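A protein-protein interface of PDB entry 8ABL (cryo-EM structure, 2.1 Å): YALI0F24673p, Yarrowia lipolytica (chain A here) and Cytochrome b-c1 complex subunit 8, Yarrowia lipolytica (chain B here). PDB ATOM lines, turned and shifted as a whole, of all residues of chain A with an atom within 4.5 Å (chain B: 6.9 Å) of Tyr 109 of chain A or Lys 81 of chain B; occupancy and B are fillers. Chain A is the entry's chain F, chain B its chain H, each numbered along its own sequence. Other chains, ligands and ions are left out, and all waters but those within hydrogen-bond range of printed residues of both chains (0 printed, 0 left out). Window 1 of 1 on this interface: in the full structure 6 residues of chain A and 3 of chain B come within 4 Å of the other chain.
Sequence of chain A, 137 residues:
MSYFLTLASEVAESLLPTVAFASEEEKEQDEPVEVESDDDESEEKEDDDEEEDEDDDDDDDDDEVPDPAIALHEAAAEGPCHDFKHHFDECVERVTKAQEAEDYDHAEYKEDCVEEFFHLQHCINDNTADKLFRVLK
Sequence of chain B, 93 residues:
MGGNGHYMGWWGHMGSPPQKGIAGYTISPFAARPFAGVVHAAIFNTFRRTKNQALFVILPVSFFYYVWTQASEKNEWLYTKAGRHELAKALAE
The side-chain sulfur (SG) of Cys 91 of chain A lies within hydrogen-bond range of the side-chain amino group (NZ) of Lys 81 of chain B, at 3.6 Å.
NZ of Lys 81 of chain B lies within salt-bridge range of OE1 of Glu 111 of chain A (2.8 Å).
NZ of Lys 81 of chain B sits at hydrogen-bond distance from O of Asp 112 of chain A.
OE2 of Glu 115 of chain A sits at hydrogen-bond distance from N of Lys 81 of chain B, at 2.9 Å.
The side-chain carboxylate (OE2) of Glu 116 of chain A lies within salt-bridge range of the side-chain amino group (NZ) of Lys 81 of chain B, at 2.9 Å.
NH2 of Arg 94 of chain A sits close to SG of Cys 91 of chain A (3.7 Å).
The guanidinium group (NH1) of Arg 94 of chain A lies within salt-bridge range of the side-chain carboxylate (OE2) of Glu 111 of chain A, 3.0 Å away.
NH2 of Arg 94 of chain A lies within salt-bridge range of OE1 of Glu 116 of chain A.
OG1 of Thr 80 of chain B is in hydrogen-bond range of O of Trp 77 of chain B, 2.7 Å away.
Lys 81 of chain B touches Tyr 109 of chain A.
Tyr 109 of chain A touches Arg 84 of chain B.
OE2 of Glu 115 of chain A touches CA of Thr 80 of chain B, 3.4 Å away.
Arg 94 of chain A touches none of the printed residues of chain B.
Tyr 109 of chain A touches just these residues of chain B: Lys 81 and Arg 84.
Printed residues of chain B within 4 Å of Glu 111 of chain A: Lys 81 (2.8 Å).
Of the printed residues of chain B, Asp 112 of chain A touches Lys 81 (3.2 Å).
Of the printed residues of chain B, Glu 115 of chain A touches Thr 80 and Lys 81.
Of the printed residues of chain B, Glu 116 of chain A touches Lys 81.
Lys 81 of chain B touches six residues of chain A.
Gly 83 of chain B touches none of the printed residues of chain A.
Of the printed residues of chain A, Arg 84 of chain B touches Tyr 109.
The nearest residue of chain A that does not touch Lys 81 of chain B is Arg 94 of chain A (4.1 Å).
Printed residues of chain B that touch a printed residue of chain A: Thr 80, Lys 81 and Arg 84.
Along chain B the printed residues that touch a printed residue of chain A span positions 80 to 84.
Among the printed residues, 8 pairs touch across the chains.
Among the printed residues, Asp or Glu carboxylates within 4 Å of a Lys or Arg side-chain nitrogen of the other chain: Glu 111 of chain A with Lys 81 of chain B and Glu 116 of chain A with Lys 81 of chain B.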
ATOM      1  N   CYS A  91      16.788  31.077  28.905  1.00  0.00           N
ATOM      2  CA  CYS A  91      17.807  30.780  27.906  1.00  0.00           C
ATOM      3  C   CYS A  91      17.956  31.959  26.947  1.00  0.00           C
ATOM      4  O   CYS A  91      19.070  32.423  26.729  1.00  0.00           O
ATOM      5  CB  CYS A  91      17.530  29.495  27.123  1.00  0.00           C
ATOM      6  SG  CYS A  91      18.810  29.095  25.893  1.00  0.00           S
ATOM      7  N   ARG A  94      19.791  34.914  28.416  1.00  0.00           N
ATOM      8  CA  ARG A  94      21.224  34.667  28.531  1.00  0.00           C
ATOM      9  C   ARG A  94      21.921  34.820  27.182  1.00  0.00           C
ATOM     10  O   ARG A  94      22.978  35.444  27.114  1.00  0.00           O
ATOM     11  CB  ARG A  94      21.536  33.278  29.103  1.00  0.00           C
ATOM     12  CG  ARG A  94      20.996  33.061  30.508  1.00  0.00           C
ATOM     13  CD  ARG A  94      21.202  31.673  31.080  1.00  0.00           C
ATOM     14  NE  ARG A  94      20.478  30.578  30.440  1.00  0.00           N
ATOM     15  CZ  ARG A  94      21.056  29.585  29.775  1.00  0.00           C
ATOM     16  NH1 ARG A  94      22.368  29.575  29.625  1.00  0.00           N
ATOM     17  NH2 ARG A  94      20.330  28.618  29.233  1.00  0.00           N
ATOM     18  N   ALA A 107      34.252  33.788  19.933  1.00  0.00           N
ATOM     19  CA  ALA A 107      34.084  32.810  20.995  1.00  0.00           C
ATOM     20  C   ALA A 107      34.128  31.406  20.398  1.00  0.00           C
ATOM     21  O   ALA A 107      33.897  31.225  19.205  1.00  0.00           O
ATOM     22  CB  ALA A 107      32.820  33.083  21.772  1.00  0.00           C
ATOM     23  N   GLU A 108      34.481  30.427  21.234  1.00  0.00           N
ATOM     24  CA  GLU A 108      34.610  29.050  20.791  1.00  0.00           C
ATOM     25  C   GLU A 108      33.207  28.459  20.677  1.00  0.00           C
ATOM     26  O   GLU A 108      32.814  27.956  19.623  1.00  0.00           O
ATOM     27  CB  GLU A 108      35.515  28.277  21.755  1.00  0.00           C
ATOM     28  CG  GLU A 108      36.020  26.950  21.206  1.00  0.00           C
ATOM     29  CD  GLU A 108      35.054  25.775  21.267  1.00  0.00           C
ATOM     30  OE1 GLU A 108      34.761  25.195  20.200  1.00  0.00           O
ATOM     31  OE2 GLU A 108      34.609  25.427  22.383  1.00  0.00           O
ATOM     32  N   TYR A 109      32.469  28.566  21.785  1.00  0.00           N
ATOM     33  CA  TYR A 109      31.139  28.001  21.918  1.00  0.00           C
ATOM     34  C   TYR A 109      30.103  29.118  21.949  1.00  0.00           C
ATOM     35  O   TYR A 109      30.102  29.939  22.869  1.00  0.00           O
ATOM     36  CB  TYR A 109      31.043  27.155  23.194  1.00  0.00           C
ATOM     37  CG  TYR A 109      29.657  26.669  23.533  1.00  0.00           C
ATOM     38  CD1 TYR A 109      28.989  25.778  22.701  1.00  0.00           C
ATOM     39  CD2 TYR A 109      29.011  27.089  24.687  1.00  0.00           C
ATOM     40  CE1 TYR A 109      27.714  25.322  23.005  1.00  0.00           C
ATOM     41  CE2 TYR A 109      27.736  26.643  25.005  1.00  0.00           C
ATOM     42  CZ  TYR A 109      27.087  25.753  24.164  1.00  0.00           C
ATOM     43  OH  TYR A 109      25.836  25.303  24.477  1.00  0.00           O
ATOM     44  N   LYS A 110      29.213  29.109  20.952  1.00  0.00           N
ATOM     45  CA  LYS A 110      28.056  29.988  20.948  1.00  0.00           C
ATOM     46  C   LYS A 110      26.806  29.169  21.271  1.00  0.00           C
ATOM     47  O   LYS A 110      26.402  28.307  20.493  1.00  0.00           O
ATOM     48  CB  LYS A 110      27.950  30.745  19.619  1.00  0.00           C
ATOM     49  CG  LYS A 110      29.162  31.576  19.222  1.00  0.00           C
ATOM     50  CD  LYS A 110      29.065  32.094  17.799  1.00  0.00           C
ATOM     51  CE  LYS A 110      30.175  33.049  17.403  1.00  0.00           C
ATOM     52  NZ  LYS A 110      31.483  32.671  17.995  1.00  0.00           N
ATOM     53  N   GLU A 111      26.207  29.445  22.435  1.00  0.00           N
ATOM     54  CA  GLU A 111      25.009  28.772  22.899  1.00  0.00           C
ATOM     55  C   GLU A 111      23.799  29.189  22.061  1.00  0.00           C
ATOM     56  O   GLU A 111      23.667  30.361  21.717  1.00  0.00           O
ATOM     57  CB  GLU A 111      24.772  29.187  24.349  1.00  0.00           C
ATOM     58  CG  GLU A 111      23.915  28.199  25.116  1.00  0.00           C
ATOM     59  CD  GLU A 111      23.167  28.777  26.310  1.00  0.00           C
ATOM     60  OE1 GLU A 111      21.992  28.377  26.534  1.00  0.00           O
ATOM     61  OE2 GLU A 111      23.743  29.643  26.995  1.00  0.00           O
ATOM     62  N   ASP A 112      22.906  28.231  21.777  1.00  0.00           N
ATOM     63  CA  ASP A 112      21.578  28.501  21.236  1.00  0.00           C
ATOM     64  C   ASP A 112      20.516  28.104  22.259  1.00  0.00           C
ATOM     65  O   ASP A 112      20.835  27.683  23.372  1.00  0.00           O
ATOM     66  CB  ASP A 112      21.329  27.775  19.909  1.00  0.00           C
ATOM     67  CG  ASP A 112      21.661  26.297  19.979  1.00  0.00           C
ATOM     68  OD1 ASP A 112      20.805  25.512  20.426  1.00  0.00           O
ATOM     69  OD2 ASP A 112      22.808  25.955  19.633  1.00  0.00           O
ATOM     70  N   GLU A 115      17.357  23.616  22.184  1.00  0.00           N
ATOM     71  CA  GLU A 115      16.973  22.521  23.065  1.00  0.00           C
ATOM     72  C   GLU A 115      15.754  22.905  23.899  1.00  0.00           C
ATOM     73  O   GLU A 115      14.780  22.154  23.961  1.00  0.00           O
ATOM     74  CB  GLU A 115      18.122  22.107  23.977  1.00  0.00           C
ATOM     75  CG  GLU A 115      18.903  20.915  23.465  1.00  0.00           C
ATOM     76  CD  GLU A 115      20.184  20.620  24.231  1.00  0.00           C
ATOM     77  OE1 GLU A 115      20.109  20.399  25.461  1.00  0.00           O
ATOM     78  OE2 GLU A 115      21.260  20.618  23.598  1.00  0.00           O
ATOM     79  N   GLU A 116      15.802  24.106  24.487  1.00  0.00           N
ATOM     80  CA  GLU A 116      14.736  24.568  25.362  1.00  0.00           C
ATOM     81  C   GLU A 116      13.463  24.812  24.560  1.00  0.00           C
ATOM     82  O   GLU A 116      12.358  24.581  25.056  1.00  0.00           O
ATOM     83  CB  GLU A 116      15.122  25.877  26.038  1.00  0.00           C
ATOM     84  CG  GLU A 116      16.014  25.667  27.242  1.00  0.00           C
ATOM     85  CD  GLU A 116      17.493  25.704  26.913  1.00  0.00           C
ATOM     86  OE1 GLU A 116      18.310  25.821  27.865  1.00  0.00           O
ATOM     87  OE2 GLU A 116      17.835  25.703  25.716  1.00  0.00           O
ATOM     88  N   TRP B  77      22.212  11.865  26.173  1.00  0.00           N
ATOM     89  CA  TRP B  77      22.704  12.902  27.062  1.00  0.00           C
ATOM     90  C   TRP B  77      23.970  13.536  26.491  1.00  0.00           C
ATOM     91  O   TRP B  77      24.206  14.724  26.685  1.00  0.00           O
ATOM     92  CB  TRP B  77      22.946  12.325  28.458  1.00  0.00           C
ATOM     93  CG  TRP B  77      23.496  13.353  29.394  1.00  0.00           C
ATOM     94  CD1 TRP B  77      22.785  14.310  30.056  1.00  0.00           C
ATOM     95  CD2 TRP B  77      24.876  13.573  29.726  1.00  0.00           C
ATOM     96  NE1 TRP B  77      23.620  15.095  30.801  1.00  0.00           N
ATOM     97  CE2 TRP B  77      24.907  14.668  30.618  1.00  0.00           C
ATOM     98  CE3 TRP B  77      26.080  12.944  29.378  1.00  0.00           C
ATOM     99  CZ2 TRP B  77      26.094  15.155  31.161  1.00  0.00           C
ATOM    100  CZ3 TRP B  77      27.255  13.421  29.921  1.00  0.00           C
ATOM    101  CH2 TRP B  77      27.255  14.511  30.797  1.00  0.00           C
ATOM    102  N   LEU B  78      24.776  12.733  25.791  1.00  0.00           N
ATOM    103  CA  LEU B  78      26.043  13.202  25.250  1.00  0.00           C
ATOM    104  C   LEU B  78      25.805  14.232  24.147  1.00  0.00           C
ATOM    105  O   LEU B  78      26.699  15.023  23.855  1.00  0.00           O
ATOM    106  CB  LEU B  78      26.832  12.016  24.681  1.00  0.00           C
ATOM    107  CG  LEU B  78      27.587  11.127  25.672  1.00  0.00           C
ATOM    108  CD1 LEU B  78      28.152   9.896  24.967  1.00  0.00           C
ATOM    109  CD2 LEU B  78      28.709  11.884  26.367  1.00  0.00           C
ATOM    110  N   TYR B  79      24.625  14.183  23.508  1.00  0.00           N
ATOM    111  CA  TYR B  79      24.311  15.046  22.378  1.00  0.00           C
ATOM    112  C   TYR B  79      23.414  16.207  22.800  1.00  0.00           C
ATOM    113  O   TYR B  79      22.791  16.846  21.957  1.00  0.00           O
ATOM    114  CB  TYR B  79      23.776  14.226  21.200  1.00  0.00           C
ATOM    115  CG  TYR B  79      24.893  13.509  20.490  1.00  0.00           C
ATOM    116  CD1 TYR B  79      25.604  14.131  19.475  1.00  0.00           C
ATOM    117  CD2 TYR B  79      25.315  12.254  20.911  1.00  0.00           C
ATOM    118  CE1 TYR B  79      26.664  13.495  18.849  1.00  0.00           C
ATOM    119  CE2 TYR B  79      26.375  11.605  20.301  1.00  0.00           C
ATOM    120  CZ  TYR B  79      27.061  12.238  19.277  1.00  0.00           C
ATOM    121  OH  TYR B  79      28.111  11.615  18.672  1.00  0.00           O
ATOM    122  N   THR B  80      23.341  16.463  24.109  1.00  0.00           N
ATOM    123  CA  THR B  80      22.743  17.688  24.617  1.00  0.00           C
ATOM    124  C   THR B  80      23.857  18.689  24.906  1.00  0.00           C
ATOM    125  O   THR B  80      25.024  18.339  24.757  1.00  0.00           O
ATOM    126  CB  THR B  80      21.858  17.402  25.833  1.00  0.00           C
ATOM    127  OG1 THR B  80      22.677  16.927  26.903  1.00  0.00           O
ATOM    128  CG2 THR B  80      20.776  16.393  25.520  1.00  0.00           C
ATOM    129  N   LYS B  81      23.482  19.922  25.295  1.00  0.00           N
ATOM    130  CA  LYS B  81      24.401  20.989  25.678  1.00  0.00           C
ATOM    131  C   LYS B  81      25.206  20.574  26.903  1.00  0.00           C
ATOM    132  O   LYS B  81      26.414  20.791  26.970  1.00  0.00           O
ATOM    133  CB  LYS B  81      23.626  22.217  26.170  1.00  0.00           C
ATOM    134  CG  LYS B  81      23.051  23.150  25.119  1.00  0.00           C
ATOM    135  CD  LYS B  81      22.560  24.453  25.742  1.00  0.00           C
ATOM    136  CE  LYS B  81      21.178  24.868  25.286  1.00  0.00           C
ATOM    137  NZ  LYS B  81      20.653  26.011  26.073  1.00  0.00           N
ATOM    138  N   ALA B  82      24.498  20.015  27.890  1.00  0.00           N
ATOM    139  CA  ALA B  82      25.071  19.557  29.144  1.00  0.00           C
ATOM    140  C   ALA B  82      26.142  18.486  28.918  1.00  0.00           C
ATOM    141  O   ALA B  82      27.075  18.370  29.713  1.00  0.00           O
ATOM    142  CB  ALA B  82      23.958  19.053  30.024  1.00  0.00           C
ATOM    143  N   GLY B  83      26.012  17.713  27.830  1.00  0.00           N
ATOM    144  CA  GLY B  83      26.901  16.588  27.577  1.00  0.00           C
ATOM    145  C   GLY B  83      28.061  16.915  26.638  1.00  0.00           C
ATOM    146  O   GLY B  83      28.750  15.998  26.185  1.00  0.00           O
ATOM    147  N   ARG B  84      28.239  18.212  26.342  1.00  0.00           N
ATOM    148  CA  ARG B  84      29.201  18.736  25.380  1.00  0.00           C
ATOM    149  C   ARG B  84      30.618  18.252  25.663  1.00  0.00           C
ATOM    150  O   ARG B  84      31.346  17.865  24.749  1.00  0.00           O
ATOM    151  CB  ARG B  84      29.339  20.242  25.580  1.00  0.00           C
ATOM    152  CG  ARG B  84      28.461  21.067  24.658  1.00  0.00           C
ATOM    153  CD  ARG B  84      29.042  22.453  24.601  1.00  0.00           C
ATOM    154  NE  ARG B  84      28.791  23.158  25.844  1.00  0.00           N
ATOM    155  CZ  ARG B  84      29.625  24.043  26.368  1.00  0.00           C
ATOM    156  NH1 ARG B  84      30.760  24.329  25.754  1.00  0.00           N
ATOM    157  NH2 ARG B  84      29.316  24.643  27.502  1.00  0.00           N
ATOM    158  N   HIS B  85      31.012  18.381  26.935  1.00  0.00           N
ATOM    159  CA  HIS B  85      32.377  18.164  27.375  1.00  0.00           C
ATOM    160  C   HIS B  85      32.697  16.679  27.373  1.00  0.00           C
ATOM    161  O   HIS B  85      33.783  16.269  26.970  1.00  0.00           O
ATOM    162  CB  HIS B  85      32.563  18.705  28.792  1.00  0.00           C
ATOM    163  CG  HIS B  85      32.177  20.136  28.920  1.00  0.00           C
ATOM    164  ND1 HIS B  85      32.853  21.139  28.257  1.00  0.00           N
ATOM    165  CD2 HIS B  85      31.182  20.732  29.610  1.00  0.00           C
ATOM    166  CE1 HIS B  85      32.301  22.299  28.547  1.00  0.00           C
ATOM    167  NE2 HIS B  85      31.271  22.076  29.374  1.00  0.00           N
ATOM    168  N   GLU B  86      31.742  15.897  27.883  1.00  0.00           N
ATOM    169  CA  GLU B  86      31.870  14.455  27.924  1.00  0.00           C
ATOM    170  C   GLU B  86      31.847  13.909  26.500  1.00  0.00           C
ATOM    171  O   GLU B  86      32.466  12.881  26.242  1.00  0.00           O
ATOM    172  CB  GLU B  86      30.773  13.840  28.789  1.00  0.00           C
ATOM    173  CG  GLU B  86      30.953  14.056  30.284  1.00  0.00           C
ATOM    174  CD  GLU B  86      30.675  15.453  30.825  1.00  0.00           C
ATOM    175  OE1 GLU B  86      29.911  16.211  30.182  1.00  0.00           O
ATOM    176  OE2 GLU B  86      31.236  15.789  31.890  1.00  0.00           O
